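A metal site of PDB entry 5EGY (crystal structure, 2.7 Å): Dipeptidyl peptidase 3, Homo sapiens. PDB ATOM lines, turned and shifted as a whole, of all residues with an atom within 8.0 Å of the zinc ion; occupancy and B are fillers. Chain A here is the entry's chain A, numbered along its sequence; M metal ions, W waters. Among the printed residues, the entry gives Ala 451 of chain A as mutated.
ND1 of His 455 lies within hydrogen-bond range of OE2 of Glu 507 (2.9 Å). The side-chain carboxylate of Glu 512 sits at hydrogen-bond distance from a ring nitrogen (ND1) of His 450, at 2.7 Å. The side-chain hydroxyl (OH) of Tyr 318 lies within hydrogen-bond range of the side-chain carboxylate (OE2) of Glu 508 (2.7 Å).
The zinc ion is bound by a ring nitrogen (NE2) of His 450 (2.0 Å), a ring nitrogen (NE2) of His 455 (2.1 Å) and the side-chain carboxylate (OE1) of Glu 508 (2.1 Å). The zinc ion has three donor atoms within binding distance. Slightly farther from the zinc ion lies water W1 (2.7 Å).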
ATOM      1  N   GLU A 316     -13.294  10.804  -7.835  1.00  0.00           N
ATOM      2  CA  GLU A 316     -13.982   9.805  -8.644  1.00  0.00           C
ATOM      3  C   GLU A 316     -13.206   9.407  -9.899  1.00  0.00           C
ATOM      4  O   GLU A 316     -12.458  10.204 -10.459  1.00  0.00           O
ATOM      5  CB  GLU A 316     -15.368  10.322  -9.046  1.00  0.00           C
ATOM      6  CG  GLU A 316     -16.283  10.649  -7.864  1.00  0.00           C
ATOM      7  CD  GLU A 316     -16.710   9.423  -7.073  1.00  0.00           C
ATOM      8  OE1 GLU A 316     -16.539   8.287  -7.573  1.00  0.00           O
ATOM      9  OE2 GLU A 316     -17.218   9.589  -5.939  1.00  0.00           O
ATOM     10  N   TYR A 318     -14.557   7.889 -13.025  1.00  0.00           N
ATOM     11  CA  TYR A 318     -15.512   7.477 -14.052  1.00  0.00           C
ATOM     12  C   TYR A 318     -14.963   7.736 -15.455  1.00  0.00           C
ATOM     13  O   TYR A 318     -15.199   6.953 -16.374  1.00  0.00           O
ATOM     14  CB  TYR A 318     -16.844   8.206 -13.878  1.00  0.00           C
ATOM     15  CG  TYR A 318     -17.606   7.845 -12.631  1.00  0.00           C
ATOM     16  CD1 TYR A 318     -18.352   6.682 -12.563  1.00  0.00           C
ATOM     17  CD2 TYR A 318     -17.594   8.683 -11.524  1.00  0.00           C
ATOM     18  CE1 TYR A 318     -19.064   6.358 -11.419  1.00  0.00           C
ATOM     19  CE2 TYR A 318     -18.299   8.366 -10.378  1.00  0.00           C
ATOM     20  CZ  TYR A 318     -19.037   7.201 -10.332  1.00  0.00           C
ATOM     21  OH  TYR A 318     -19.735   6.877  -9.187  1.00  0.00           O
ATOM     22  N   PRO A 387     -23.751  15.334  -9.376  1.00  0.00           N
ATOM     23  CA  PRO A 387     -24.530  14.141  -9.037  1.00  0.00           C
ATOM     24  C   PRO A 387     -25.687  14.463  -8.099  1.00  0.00           C
ATOM     25  O   PRO A 387     -25.835  15.611  -7.668  1.00  0.00           O
ATOM     26  CB  PRO A 387     -23.511  13.258  -8.337  1.00  0.00           C
ATOM     27  CG  PRO A 387     -22.623  14.231  -7.635  1.00  0.00           C
ATOM     28  CD  PRO A 387     -22.539  15.446  -8.549  1.00  0.00           C
ATOM     29  N   GLY A 389     -26.353  12.305  -5.284  1.00  0.00           N
ATOM     30  CA  GLY A 389     -25.844  11.915  -3.983  1.00  0.00           C
ATOM     31  C   GLY A 389     -24.438  11.372  -4.106  1.00  0.00           C
ATOM     32  O   GLY A 389     -24.033  10.931  -5.182  1.00  0.00           O
ATOM     33  N   ILE A 390     -23.684  11.417  -3.014  1.00  0.00           N
ATOM     34  CA  ILE A 390     -22.304  10.953  -3.024  1.00  0.00           C
ATOM     35  C   ILE A 390     -21.962  10.116  -1.793  1.00  0.00           C
ATOM     36  O   ILE A 390     -22.421  10.418  -0.694  1.00  0.00           O
ATOM     37  CB  ILE A 390     -21.289  12.126  -3.105  1.00  0.00           C
ATOM     38  CG1 ILE A 390     -21.731  13.174  -4.124  1.00  0.00           C
ATOM     39  CG2 ILE A 390     -19.901  11.619  -3.446  1.00  0.00           C
ATOM     40  CD1 ILE A 390     -20.794  14.360  -4.234  1.00  0.00           C
ATOM     41  N   ASN A 391     -21.183   9.067  -1.991  1.00  0.00           N
ATOM     42  CA  ASN A 391     -20.585   8.317  -0.899  1.00  0.00           C
ATOM     43  C   ASN A 391     -19.075   8.541  -0.897  1.00  0.00           C
ATOM     44  O   ASN A 391     -18.391   8.177  -1.854  1.00  0.00           O
ATOM     45  CB  ASN A 391     -20.911   6.827  -0.996  1.00  0.00           C
ATOM     46  CG  ASN A 391     -20.270   6.013   0.121  1.00  0.00           C
ATOM     47  OD1 ASN A 391     -19.095   5.644   0.041  1.00  0.00           O
ATOM     48  ND2 ASN A 391     -21.037   5.717   1.158  1.00  0.00           N
ATOM     49  N   VAL A 447     -32.048   7.242  -3.553  1.00  0.00           N
ATOM     50  CA  VAL A 447     -30.785   7.905  -3.271  1.00  0.00           C
ATOM     51  C   VAL A 447     -30.286   7.596  -1.865  1.00  0.00           C
ATOM     52  O   VAL A 447     -29.084   7.377  -1.655  1.00  0.00           O
ATOM     53  CB  VAL A 447     -30.920   9.444  -3.448  1.00  0.00           C
ATOM     54  CG1 VAL A 447     -29.809  10.187  -2.712  1.00  0.00           C
ATOM     55  CG2 VAL A 447     -30.909   9.799  -4.927  1.00  0.00           C
ATOM     56  N   HIS A 450     -29.136   3.995  -1.833  1.00  0.00           N
ATOM     57  CA  HIS A 450     -28.018   3.884  -2.766  1.00  0.00           C
ATOM     58  C   HIS A 450     -26.679   4.152  -2.071  1.00  0.00           C
ATOM     59  O   HIS A 450     -25.693   3.458  -2.325  1.00  0.00           O
ATOM     60  CB  HIS A 450     -28.208   4.868  -3.934  1.00  0.00           C
ATOM     61  CG  HIS A 450     -27.111   4.830  -4.951  1.00  0.00           C
ATOM     62  ND1 HIS A 450     -27.259   4.221  -6.185  1.00  0.00           N
ATOM     63  CD2 HIS A 450     -25.861   5.338  -4.939  1.00  0.00           C
ATOM     64  CE1 HIS A 450     -26.150   4.352  -6.877  1.00  0.00           C
ATOM     65  NE2 HIS A 450     -25.271   5.024  -6.143  1.00  0.00           N
ATOM     66  N   ALA A 451     -26.665   5.158  -1.209  1.00  0.00           N
ATOM     67  CA  ALA A 451     -25.426   5.567  -0.560  1.00  0.00           C
ATOM     68  C   ALA A 451     -25.195   4.857   0.764  1.00  0.00           C
ATOM     69  O   ALA A 451     -24.149   4.258   0.982  1.00  0.00           O
ATOM     70  CB  ALA A 451     -25.414   7.078  -0.349  1.00  0.00           C
ATOM     71  N   GLY A 454     -25.993   0.917   0.206  1.00  0.00           N
ATOM     72  CA  GLY A 454     -25.435   0.431  -1.045  1.00  0.00           C
ATOM     73  C   GLY A 454     -23.916   0.504  -1.052  1.00  0.00           C
ATOM     74  O   GLY A 454     -23.250  -0.518  -0.954  1.00  0.00           O
ATOM     75  N   HIS A 455     -23.389   1.716  -1.182  1.00  0.00           N
ATOM     76  CA  HIS A 455     -21.935   1.922  -1.175  1.00  0.00           C
ATOM     77  C   HIS A 455     -21.353   1.705   0.226  1.00  0.00           C
ATOM     78  O   HIS A 455     -20.176   1.356   0.369  1.00  0.00           O
ATOM     79  CB  HIS A 455     -21.573   3.317  -1.673  1.00  0.00           C
ATOM     80  CG  HIS A 455     -21.922   3.570  -3.103  1.00  0.00           C
ATOM     81  ND1 HIS A 455     -21.428   2.813  -4.138  1.00  0.00           N
ATOM     82  CD2 HIS A 455     -22.712   4.520  -3.678  1.00  0.00           C
ATOM     83  CE1 HIS A 455     -21.893   3.272  -5.285  1.00  0.00           C
ATOM     84  NE2 HIS A 455     -22.672   4.306  -5.030  1.00  0.00           N
ATOM     85  N   SER A 504     -16.271   0.966 -11.750  1.00  0.00           N
ATOM     86  CA  SER A 504     -17.263   2.012 -11.505  1.00  0.00           C
ATOM     87  C   SER A 504     -18.685   1.497 -11.750  1.00  0.00           C
ATOM     88  O   SER A 504     -19.569   1.675 -10.909  1.00  0.00           O
ATOM     89  CB  SER A 504     -16.982   3.234 -12.373  1.00  0.00           C
ATOM     90  OG  SER A 504     -15.800   3.907 -11.944  1.00  0.00           O
ATOM     91  N   GLU A 507     -19.962  -1.430  -9.205  1.00  0.00           N
ATOM     92  CA  GLU A 507     -20.288  -0.989  -7.848  1.00  0.00           C
ATOM     93  C   GLU A 507     -21.598  -0.195  -7.780  1.00  0.00           C
ATOM     94  O   GLU A 507     -22.358  -0.330  -6.824  1.00  0.00           O
ATOM     95  CB  GLU A 507     -19.148  -0.164  -7.255  1.00  0.00           C
ATOM     96  CG  GLU A 507     -19.491   0.556  -5.958  1.00  0.00           C
ATOM     97  CD  GLU A 507     -19.853  -0.389  -4.820  1.00  0.00           C
ATOM     98  OE1 GLU A 507     -19.541  -1.584  -4.899  1.00  0.00           O
ATOM     99  OE2 GLU A 507     -20.455   0.086  -3.832  1.00  0.00           O
ATOM    100  N   GLU A 508     -21.845   0.629  -8.794  1.00  0.00           N
ATOM    101  CA  GLU A 508     -23.094   1.383  -8.840  1.00  0.00           C
ATOM    102  C   GLU A 508     -24.277   0.424  -9.025  1.00  0.00           C
ATOM    103  O   GLU A 508     -25.332   0.614  -8.431  1.00  0.00           O
ATOM    104  CB  GLU A 508     -23.081   2.424  -9.957  1.00  0.00           C
ATOM    105  CG  GLU A 508     -22.021   3.514  -9.811  1.00  0.00           C
ATOM    106  CD  GLU A 508     -22.161   4.339  -8.534  1.00  0.00           C
ATOM    107  OE1 GLU A 508     -23.292   4.463  -8.002  1.00  0.00           O
ATOM    108  OE2 GLU A 508     -21.125   4.859  -8.066  1.00  0.00           O
ATOM    109  N   CYS A 509     -24.058  -0.612  -9.839  1.00  0.00           N
ATOM    110  CA  CYS A 509     -25.076  -1.632 -10.079  1.00  0.00           C
ATOM    111  C   CYS A 509     -25.415  -2.392  -8.808  1.00  0.00           C
ATOM    112  O   CYS A 509     -26.560  -2.748  -8.561  1.00  0.00           O
ATOM    113  CB  CYS A 509     -24.612  -2.604 -11.162  1.00  0.00           C
ATOM    114  SG  CYS A 509     -25.798  -3.914 -11.566  1.00  0.00           S
ATOM    115  N   ALA A 511     -25.011  -1.057  -5.873  1.00  0.00           N
ATOM    116  CA  ALA A 511     -25.661  -0.038  -5.060  1.00  0.00           C
ATOM    117  C   ALA A 511     -27.098   0.183  -5.511  1.00  0.00           C
ATOM    118  O   ALA A 511     -28.009   0.306  -4.684  1.00  0.00           O
ATOM    119  CB  ALA A 511     -24.882   1.266  -5.130  1.00  0.00           C
ATOM    120  N   GLU A 512     -27.305   0.232  -6.827  1.00  0.00           N
ATOM    121  CA  GLU A 512     -28.633   0.422  -7.398  1.00  0.00           C
ATOM    122  C   GLU A 512     -29.569  -0.732  -7.052  1.00  0.00           C
ATOM    123  O   GLU A 512     -30.739  -0.508  -6.731  1.00  0.00           O
ATOM    124  CB  GLU A 512     -28.547   0.571  -8.921  1.00  0.00           C
ATOM    125  CG  GLU A 512     -28.079   1.939  -9.393  1.00  0.00           C
ATOM    126  CD  GLU A 512     -29.053   3.054  -9.046  1.00  0.00           C
ATOM    127  OE1 GLU A 512     -29.610   3.673  -9.976  1.00  0.00           O
ATOM    128  OE2 GLU A 512     -29.253   3.295  -7.835  1.00  0.00           O
ATOM    129  N   HIS A 568     -23.359   4.573 -14.644  1.00  0.00           N
ATOM    130  CA  HIS A 568     -24.657   4.443 -13.996  1.00  0.00           C
ATOM    131  C   HIS A 568     -25.703   3.867 -14.936  1.00  0.00           C
ATOM    132  O   HIS A 568     -26.576   3.106 -14.523  1.00  0.00           O
ATOM    133  CB  HIS A 568     -25.130   5.797 -13.463  1.00  0.00           C
ATOM    134  CG  HIS A 568     -24.214   6.411 -12.453  1.00  0.00           C
ATOM    135  ND1 HIS A 568     -22.992   6.962 -12.792  1.00  0.00           N
ATOM    136  CD2 HIS A 568     -24.330   6.559 -11.110  1.00  0.00           C
ATOM    137  CE1 HIS A 568     -22.401   7.429 -11.703  1.00  0.00           C
ATOM    138  NE2 HIS A 568     -23.189   7.185 -10.674  1.00  0.00           N
ATOM    139  N   ARG A 572     -27.903   0.154 -14.989  1.00  0.00           N
ATOM    140  CA  ARG A 572     -29.357   0.029 -15.026  1.00  0.00           C
ATOM    141  C   ARG A 572     -29.820  -0.849 -16.182  1.00  0.00           C
ATOM    142  O   ARG A 572     -30.865  -1.504 -16.096  1.00  0.00           O
ATOM    143  CB  ARG A 572     -30.001   1.414 -15.109  1.00  0.00           C
ATOM    144  CG  ARG A 572     -29.666   2.261 -13.901  1.00  0.00           C
ATOM    145  CD  ARG A 572     -30.062   3.712 -14.075  1.00  0.00           C
ATOM    146  NE  ARG A 572     -29.411   4.532 -13.067  1.00  0.00           N
ATOM    147  CZ  ARG A 572     -29.556   5.855 -12.961  1.00  0.00           C
ATOM    148  NH1 ARG A 572     -30.341   6.507 -13.813  1.00  0.00           N
ATOM    149  NH2 ARG A 572     -28.915   6.516 -12.016  1.00  0.00           N
HETATM  150 ZN    ZN M   1     -23.383   5.739  -6.354  1.00  0.00          ZN
HETATM  151  O   HOH W   1     -23.965   8.310  -6.975  1.00  0.00           O
